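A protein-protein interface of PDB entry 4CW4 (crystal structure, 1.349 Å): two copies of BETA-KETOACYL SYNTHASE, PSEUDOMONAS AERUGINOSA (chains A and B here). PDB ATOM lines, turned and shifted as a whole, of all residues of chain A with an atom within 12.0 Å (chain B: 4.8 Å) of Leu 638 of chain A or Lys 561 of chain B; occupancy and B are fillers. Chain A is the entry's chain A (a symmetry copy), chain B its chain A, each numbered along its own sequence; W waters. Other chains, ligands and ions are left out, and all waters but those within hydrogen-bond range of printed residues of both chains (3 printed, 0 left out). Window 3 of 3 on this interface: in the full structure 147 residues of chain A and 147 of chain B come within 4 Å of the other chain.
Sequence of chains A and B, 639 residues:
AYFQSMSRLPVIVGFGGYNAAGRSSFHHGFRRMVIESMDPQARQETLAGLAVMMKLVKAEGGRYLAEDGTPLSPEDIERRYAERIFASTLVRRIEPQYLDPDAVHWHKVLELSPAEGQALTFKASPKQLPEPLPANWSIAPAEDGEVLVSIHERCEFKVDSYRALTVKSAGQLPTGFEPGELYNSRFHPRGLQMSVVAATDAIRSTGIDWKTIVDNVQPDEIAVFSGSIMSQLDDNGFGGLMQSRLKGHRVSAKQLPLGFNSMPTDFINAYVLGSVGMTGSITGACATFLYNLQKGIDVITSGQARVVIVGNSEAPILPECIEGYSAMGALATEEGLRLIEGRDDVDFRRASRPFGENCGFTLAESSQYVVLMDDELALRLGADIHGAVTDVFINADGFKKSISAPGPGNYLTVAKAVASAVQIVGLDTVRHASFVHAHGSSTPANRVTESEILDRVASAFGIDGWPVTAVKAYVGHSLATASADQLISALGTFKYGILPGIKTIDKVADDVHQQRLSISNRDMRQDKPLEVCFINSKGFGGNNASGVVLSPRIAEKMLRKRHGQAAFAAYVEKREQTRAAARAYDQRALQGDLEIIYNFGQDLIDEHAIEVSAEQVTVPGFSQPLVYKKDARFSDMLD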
ATOM      1  N   LYS A 629      -1.412  34.614 -10.786  1.00  0.00           N
ATOM      2  CA  LYS A 629      -2.566  35.457 -10.495  1.00  0.00           C
ATOM      3  C   LYS A 629      -3.819  34.662 -10.164  1.00  0.00           C
ATOM      4  O   LYS A 629      -4.177  33.711 -10.856  1.00  0.00           O
ATOM      5  CB  LYS A 629      -2.817  36.428 -11.655  1.00  0.00           C
ATOM      6  CG  LYS A 629      -1.801  37.571 -11.698  1.00  0.00           C
ATOM      7  CD  LYS A 629      -2.084  38.547 -12.828  1.00  0.00           C
ATOM      8  CE  LYS A 629      -1.341  39.864 -12.641  1.00  0.00           C
ATOM      9  NZ  LYS A 629       0.121  39.778 -12.930  1.00  0.00           N
ATOM     10  N   LYS A 630      -4.474  35.058  -9.079  1.00  0.00           N
ATOM     11  CA  LYS A 630      -5.753  34.480  -8.690  1.00  0.00           C
ATOM     12  C   LYS A 630      -6.803  34.796  -9.751  1.00  0.00           C
ATOM     13  O   LYS A 630      -6.950  35.942 -10.163  1.00  0.00           O
ATOM     14  CB  LYS A 630      -6.188  35.037  -7.328  1.00  0.00           C
ATOM     15  CG  LYS A 630      -7.572  34.593  -6.861  1.00  0.00           C
ATOM     16  CD  LYS A 630      -7.569  33.146  -6.392  1.00  0.00           C
ATOM     17  CE  LYS A 630      -8.867  32.779  -5.648  1.00  0.00           C
ATOM     18  NZ  LYS A 630     -10.061  32.640  -6.543  1.00  0.00           N
ATOM     19  N   ASP A 631      -7.541  33.767 -10.154  1.00  0.00           N
ATOM     20  CA  ASP A 631      -8.523  33.825 -11.229  1.00  0.00           C
ATOM     21  C   ASP A 631      -9.933  33.820 -10.634  1.00  0.00           C
ATOM     22  O   ASP A 631     -10.244  32.971  -9.804  1.00  0.00           O
ATOM     23  CB  ASP A 631      -8.334  32.583 -12.107  1.00  0.00           C
ATOM     24  CG  ASP A 631      -9.190  32.601 -13.345  1.00  0.00           C
ATOM     25  OD1 ASP A 631      -9.729  33.678 -13.685  1.00  0.00           O
ATOM     26  OD2 ASP A 631      -9.303  31.533 -13.988  1.00  0.00           O
ATOM     27  N   ALA A 632     -10.772  34.773 -11.038  1.00  0.00           N
ATOM     28  CA  ALA A 632     -12.175  34.795 -10.614  1.00  0.00           C
ATOM     29  C   ALA A 632     -13.130  34.656 -11.796  1.00  0.00           C
ATOM     30  O   ALA A 632     -14.346  34.711 -11.620  1.00  0.00           O
ATOM     31  CB  ALA A 632     -12.476  36.071  -9.840  1.00  0.00           C
ATOM     32  N   ARG A 633     -12.589  34.463 -12.995  1.00  0.00           N
ATOM     33  CA  ARG A 633     -13.416  34.442 -14.198  1.00  0.00           C
ATOM     34  C   ARG A 633     -14.536  33.411 -14.157  1.00  0.00           C
ATOM     35  O   ARG A 633     -15.647  33.698 -14.588  1.00  0.00           O
ATOM     36  CB  ARG A 633     -12.551  34.198 -15.437  1.00  0.00           C
ATOM     37  CG  ARG A 633     -11.667  35.385 -15.799  1.00  0.00           C
ATOM     38  CD  ARG A 633     -10.668  35.039 -16.888  1.00  0.00           C
ATOM     39  NE  ARG A 633      -9.928  33.854 -16.498  1.00  0.00           N
ATOM     40  CZ  ARG A 633      -9.231  33.073 -17.317  1.00  0.00           C
ATOM     41  NH1 ARG A 633      -9.128  33.344 -18.619  1.00  0.00           N
ATOM     42  NH2 ARG A 633      -8.631  32.008 -16.817  1.00  0.00           N
ATOM     43  N   PHE A 634     -14.243  32.210 -13.657  1.00  0.00           N
ATOM     44  CA  PHE A 634     -15.151  31.073 -13.800  1.00  0.00           C
ATOM     45  C   PHE A 634     -15.531  30.466 -12.458  1.00  0.00           C
ATOM     46  O   PHE A 634     -16.025  29.342 -12.398  1.00  0.00           O
ATOM     47  CB  PHE A 634     -14.522  30.004 -14.705  1.00  0.00           C
ATOM     48  CG  PHE A 634     -13.937  30.554 -15.974  1.00  0.00           C
ATOM     49  CD1 PHE A 634     -14.726  31.279 -16.853  1.00  0.00           C
ATOM     50  CD2 PHE A 634     -12.598  30.369 -16.283  1.00  0.00           C
ATOM     51  CE1 PHE A 634     -14.192  31.816 -18.012  1.00  0.00           C
ATOM     52  CE2 PHE A 634     -12.062  30.891 -17.456  1.00  0.00           C
ATOM     53  CZ  PHE A 634     -12.868  31.611 -18.327  1.00  0.00           C
ATOM     54  N   SER A 635     -15.324  31.228 -11.393  1.00  0.00           N
ATOM     55  CA  SER A 635     -15.571  30.748 -10.036  1.00  0.00           C
ATOM     56  C   SER A 635     -16.995  30.262  -9.828  1.00  0.00           C
ATOM     57  O   SER A 635     -17.212  29.321  -9.075  1.00  0.00           O
ATOM     58  CB  SER A 635     -15.252  31.856  -9.032  1.00  0.00           C
ATOM     59  OG  SER A 635     -13.913  32.256  -9.208  1.00  0.00           O
ATOM     60  N   ASP A 636     -17.951  30.893 -10.509  1.00  0.00           N
ATOM     61  CA  ASP A 636     -19.352  30.492 -10.432  1.00  0.00           C
ATOM     62  C   ASP A 636     -19.661  29.203 -11.187  1.00  0.00           C
ATOM     63  O   ASP A 636     -20.770  28.683 -11.090  1.00  0.00           O
ATOM     64  CB  ASP A 636     -20.268  31.593 -10.969  1.00  0.00           C
ATOM     65  CG  ASP A 636     -20.057  31.863 -12.441  1.00  0.00           C
ATOM     66  OD1 ASP A 636     -18.891  32.075 -12.846  1.00  0.00           O
ATOM     67  OD2 ASP A 636     -21.061  31.867 -13.188  1.00  0.00           O
ATOM     68  N   MET A 637     -18.693  28.692 -11.941  1.00  0.00           N
ATOM     69  CA  MET A 637     -18.885  27.472 -12.706  1.00  0.00           C
ATOM     70  C   MET A 637     -18.312  26.272 -11.966  1.00  0.00           C
ATOM     71  O   MET A 637     -18.370  25.160 -12.472  1.00  0.00           O
ATOM     72  CB  MET A 637     -18.194  27.590 -14.070  1.00  0.00           C
ATOM     73  CG  MET A 637     -18.510  28.854 -14.831  1.00  0.00           C
ATOM     74  SD  MET A 637     -17.817  28.865 -16.496  1.00  0.00           S
ATOM     75  CE  MET A 637     -19.204  28.231 -17.438  1.00  0.00           C
ATOM     76  N   LEU A 638     -17.758  26.496 -10.776  1.00  0.00           N
ATOM     77  CA  LEU A 638     -16.994  25.472 -10.063  1.00  0.00           C
ATOM     78  C   LEU A 638     -17.667  25.033  -8.767  1.00  0.00           C
ATOM     79  O   LEU A 638     -18.565  25.706  -8.282  1.00  0.00           O
ATOM     80  CB  LEU A 638     -15.596  25.998  -9.747  1.00  0.00           C
ATOM     81  CG  LEU A 638     -14.831  26.581 -10.937  1.00  0.00           C
ATOM     82  CD1 LEU A 638     -13.510  27.191 -10.506  1.00  0.00           C
ATOM     83  CD2 LEU A 638     -14.599  25.511 -11.993  1.00  0.00           C
ATOM     84  N   ASP A 639     -17.185  23.907  -8.237  1.00  0.00           N
ATOM     85  CA  ASP A 639     -17.586  23.304  -6.952  1.00  0.00           C
ATOM     86  C   ASP A 639     -18.708  22.286  -7.138  1.00  0.00           C
ATOM     87  O   ASP A 639     -18.457  21.153  -7.552  1.00  0.00           O
ATOM     88  CB  ASP A 639     -17.982  24.341  -5.893  1.00  0.00           C
ATOM     89  CG  ASP A 639     -16.909  25.390  -5.667  1.00  0.00           C
ATOM     90  OD1 ASP A 639     -15.734  25.129  -6.002  1.00  0.00           O
ATOM     91  OD2 ASP A 639     -17.247  26.475  -5.140  1.00  0.00           O
ATOM     92  N   GLN B 423      -6.203  26.057 -10.498  1.00  0.00           N
ATOM     93  CA  GLN B 423      -7.274  26.896  -9.975  1.00  0.00           C
ATOM     94  C   GLN B 423      -8.641  26.469 -10.475  1.00  0.00           C
ATOM     95  O   GLN B 423      -9.641  26.661  -9.794  1.00  0.00           O
ATOM     96  CB  GLN B 423      -7.055  28.354 -10.361  1.00  0.00           C
ATOM     97  CG  GLN B 423      -5.794  28.960  -9.803  1.00  0.00           C
ATOM     98  CD  GLN B 423      -5.851  30.461  -9.823  1.00  0.00           C
ATOM     99  OE1 GLN B 423      -5.047  31.131 -10.493  1.00  0.00           O
ATOM    100  NE2 GLN B 423      -6.810  31.011  -9.088  1.00  0.00           N
ATOM    101  N   ILE B 424      -8.693  25.906 -11.674  1.00  0.00           N
ATOM    102  CA  ILE B 424      -9.970  25.620 -12.305  1.00  0.00           C
ATOM    103  C   ILE B 424     -10.446  24.199 -12.036  1.00  0.00           C
ATOM    104  O   ILE B 424     -11.615  24.009 -11.740  1.00  0.00           O
ATOM    105  CB  ILE B 424      -9.938  25.931 -13.824  1.00  0.00           C
ATOM    106  CG1 ILE B 424      -9.803  27.447 -14.037  1.00  0.00           C
ATOM    107  CG2 ILE B 424     -11.201  25.401 -14.506  1.00  0.00           C
ATOM    108  CD1 ILE B 424      -9.504  27.886 -15.483  1.00  0.00           C
ATOM    109  N   LYS B 557     -19.693  20.187 -17.096  1.00  0.00           N
ATOM    110  CA  LYS B 557     -19.924  20.400 -15.663  1.00  0.00           C
ATOM    111  C   LYS B 557     -19.989  21.905 -15.369  1.00  0.00           C
ATOM    112  O   LYS B 557     -20.848  22.372 -14.637  1.00  0.00           O
ATOM    113  CB  LYS B 557     -18.792  19.808 -14.830  1.00  0.00           C
ATOM    114  CG  LYS B 557     -18.852  18.319 -14.603  1.00  0.00           C
ATOM    115  CD  LYS B 557     -17.700  17.838 -13.703  1.00  0.00           C
ATOM    116  CE  LYS B 557     -17.655  18.598 -12.375  1.00  0.00           C
ATOM    117  NZ  LYS B 557     -16.679  18.021 -11.402  1.00  0.00           N
ATOM    118  N   MET B 558     -19.072  22.666 -15.953  1.00  0.00           N
ATOM    119  CA  MET B 558     -19.030  24.096 -15.742  1.00  0.00           C
ATOM    120  C   MET B 558     -20.283  24.799 -16.269  1.00  0.00           C
ATOM    121  O   MET B 558     -20.839  25.645 -15.576  1.00  0.00           O
ATOM    122  CB  MET B 558     -17.747  24.669 -16.364  1.00  0.00           C
ATOM    123  CG  MET B 558     -16.494  24.212 -15.621  1.00  0.00           C
ATOM    124  SD  MET B 558     -14.930  24.622 -16.435  1.00  0.00           S
ATOM    125  CE  MET B 558     -14.790  26.377 -16.045  1.00  0.00           C
ATOM    126  N   LEU B 559     -20.745  24.449 -17.464  1.00  0.00           N
ATOM    127  CA  LEU B 559     -21.953  25.079 -18.018  1.00  0.00           C
ATOM    128  C   LEU B 559     -23.192  24.714 -17.205  1.00  0.00           C
ATOM    129  O   LEU B 559     -24.078  25.564 -16.980  1.00  0.00           O
ATOM    130  CB  LEU B 559     -22.149  24.705 -19.497  1.00  0.00           C
ATOM    131  CG  LEU B 559     -21.582  25.738 -20.492  1.00  0.00           C
ATOM    132  CD1 LEU B 559     -20.058  25.717 -20.475  1.00  0.00           C
ATOM    133  CD2 LEU B 559     -22.130  25.509 -21.885  1.00  0.00           C
ATOM    134  N   ARG B 560     -23.255  23.461 -16.757  1.00  0.00           N
ATOM    135  CA  ARG B 560     -24.352  23.012 -15.902  1.00  0.00           C
ATOM    136  C   ARG B 560     -24.389  23.808 -14.600  1.00  0.00           C
ATOM    137  O   ARG B 560     -25.456  24.223 -14.143  1.00  0.00           O
ATOM    138  CB  ARG B 560     -24.230  21.513 -15.594  1.00  0.00           C
ATOM    139  CG  ARG B 560     -24.666  20.578 -16.727  1.00  0.00           C
ATOM    140  CD  ARG B 560     -24.345  19.116 -16.396  1.00  0.00           C
ATOM    141  NE  ARG B 560     -24.793  18.166 -17.415  1.00  0.00           N
ATOM    142  CZ  ARG B 560     -26.037  17.697 -17.517  1.00  0.00           C
ATOM    143  NH1 ARG B 560     -26.983  18.105 -16.677  1.00  0.00           N
ATOM    144  NH2 ARG B 560     -26.339  16.828 -18.472  1.00  0.00           N
ATOM    145  N   LYS B 561     -23.222  24.024 -14.002  1.00  0.00           N
ATOM    146  CA  LYS B 561     -23.148  24.744 -12.733  1.00  0.00           C
ATOM    147  C   LYS B 561     -23.582  26.195 -12.900  1.00  0.00           C
ATOM    148  O   LYS B 561     -24.349  26.714 -12.092  1.00  0.00           O
ATOM    149  CB  LYS B 561     -21.731  24.661 -12.161  1.00  0.00           C
ATOM    150  CG  LYS B 561     -21.515  25.408 -10.850  1.00  0.00           C
ATOM    151  CD  LYS B 561     -22.362  24.853  -9.735  1.00  0.00           C
ATOM    152  CE  LYS B 561     -21.898  25.400  -8.393  1.00  0.00           C
ATOM    153  NZ  LYS B 561     -22.941  25.236  -7.352  1.00  0.00           N
ATOM    154  N   ARG B 562     -23.095  26.850 -13.948  1.00  0.00           N
ATOM    155  CA  ARG B 562     -23.423  28.254 -14.168  1.00  0.00           C
ATOM    156  C   ARG B 562     -24.877  28.453 -14.577  1.00  0.00           C
ATOM    157  O   ARG B 562     -25.538  29.332 -14.049  1.00  0.00           O
ATOM    158  CB  ARG B 562     -22.506  28.872 -15.224  1.00  0.00           C
ATOM    159  CG  ARG B 562     -22.926  30.268 -15.656  1.00  0.00           C
ATOM    160  CD  ARG B 562     -21.896  30.886 -16.618  1.00  0.00           C
ATOM    161  NE  ARG B 562     -20.739  31.405 -15.897  1.00  0.00           N
ATOM    162  CZ  ARG B 562     -19.655  31.898 -16.472  1.00  0.00           C
ATOM    163  NH1 ARG B 562     -19.540  31.890 -17.793  1.00  0.00           N
ATOM    164  NH2 ARG B 562     -18.674  32.383 -15.721  1.00  0.00           N
ATOM    165  N   HIS B 563     -25.377  27.634 -15.501  1.00  0.00           N
ATOM    166  CA  HIS B 563     -26.656  27.925 -16.149  1.00  0.00           C
ATOM    167  C   HIS B 563     -27.849  27.180 -15.571  1.00  0.00           C
ATOM    168  O   HIS B 563     -28.979  27.585 -15.816  1.00  0.00           O
ATOM    169  CB  HIS B 563     -26.538  27.676 -17.655  1.00  0.00           C
ATOM    170  CG  HIS B 563     -25.541  28.568 -18.318  1.00  0.00           C
ATOM    171  ND1 HIS B 563     -25.798  29.893 -18.587  1.00  0.00           N
ATOM    172  CD2 HIS B 563     -24.287  28.325 -18.765  1.00  0.00           C
ATOM    173  CE1 HIS B 563     -24.742  30.427 -19.174  1.00  0.00           C
ATOM    174  NE2 HIS B 563     -23.812  29.497 -19.289  1.00  0.00           N
ATOM    175  N   GLY B 564     -27.595  26.097 -14.840  1.00  0.00           N
ATOM    176  CA  GLY B 564     -28.659  25.345 -14.166  1.00  0.00           C
ATOM    177  C   GLY B 564     -29.245  24.212 -14.994  1.00  0.00           C
ATOM    178  O   GLY B 564     -29.093  24.161 -16.216  1.00  0.00           O
HETATM  179  O   HOH W   1      -2.729  30.638 -11.500  1.00  0.00           O
HETATM  180  O   HOH W   2     -21.884  34.367 -14.622  1.00  0.00           O
HETATM  181  O   HOH W   3      -8.608  30.247  -7.543  1.00  0.00           O
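The guanidinium group (NH2) of Arg 562 of chain B lies within hydrogen-bond range of the backbone carbonyl oxygen (O) of Arg 633 of chain A, at 3.5 Å.
SD of Met 637 of chain A sits close to NH2 of Arg 562 of chain B (3.7 Å).
The guanidinium group (NE) of Arg 562 of chain B is in salt-bridge range of the side-chain carboxylate (OD2) of Asp 636 of chain A.
The side-chain amide nitrogen (NE2) of Gln 423 of chain B sits close to the backbone NH (N) of Asp 631 of chain A.
The side-chain amide oxygen (OE1) of Gln 423 of chain B sits close to the backbone carbonyl oxygen (O) of Lys 629 of chain A (2.7 Å).
OD1 of Asp 631 of chain A is in salt-bridge range of NE of Arg 633 of chain A.
CD of Lys 630 of chain A touches NE2 of Gln 423 of chain B, at 3.5 Å.
CD1 of Ile 424 of chain B touches OD2 of Asp 631 of chain A, 3.9 Å away.
CE of Met 558 of chain B touches CB of Phe 634 of chain A (3.9 Å).
Asp 636 of chain A touches Lys 561 of chain B (O to CG, 3.4 Å).
Met 637 of chain A touches Met 558 of chain B.
Met 637 of chain A touches Lys 561 of chain B.
Leu 638 of chain A touches Gln 423 of chain B (CD1 to O, 3.97 Å).
Ile 424 of chain B touches Leu 638 of chain A (O to CD2, 3.4 Å).
Lys 561 of chain B touches Leu 638 of chain A (CE to O, 3.3 Å).
Leu 638 of chain A touches just these residues of chain B: Gln 423, Ile 424 and Lys 561.
Of chain A, only Asp 636, Met 637 and Leu 638 come within 4 Å of Lys 561 of chain B.
Ile 424 of chain B touches just these residues of chain A: Asp 631 (3.9 Å) and Leu 638 (3.4 Å).
Of chain A, only Phe 634 (3.9 Å) and Met 637 (3.5 Å) come within 4 Å of Met 558 of chain B.
No residue of chain A comes within 4 Å of His 563 of chain B.
No residue of chain A comes within 4 Å of Gly 564 of chain B.
Of the printed residues of chain B, Phe 634 of chain A touches Met 558.
Printed residues of chain B within 4 Å of Asp 631 of chain A: Gln 423 and Ile 424.
Of the printed residues of chain A, Gln 423 of chain B touches Lys 629, Lys 630, Asp 631 and Leu 638.
Lys 557 of chain B touches none of the printed residues of chain A.
Arg 560 of chain B touches none of the printed residues of chain A.
Among the printed residues, 14 pairs touch across the chains.
Among the printed residues, Asp or Glu carboxylates within 4 Å of a Lys or Arg side-chain nitrogen of the other chain: Asp 636 of chain A with Arg 562 of chain B (2.8 Å).
No position is printed for both chains.
Of the 14 pairs that touch across the chains among the printed residues, none has its exchanged pair printed and touching as well.
Water W3 lies within hydrogen-bond range of NE2 of Gln 423 of chain B and NZ of Lys 630 of chain A.
Water W1 bridges OE1 of Gln 423 of chain B and O of Lys 629 of chain A.
Water W2 lies within hydrogen-bond range of the side-chain carboxylate of Asp 636 of chain A (3.0 Å) and the guanidinium group of Arg 562 of chain B (3.4 Å).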
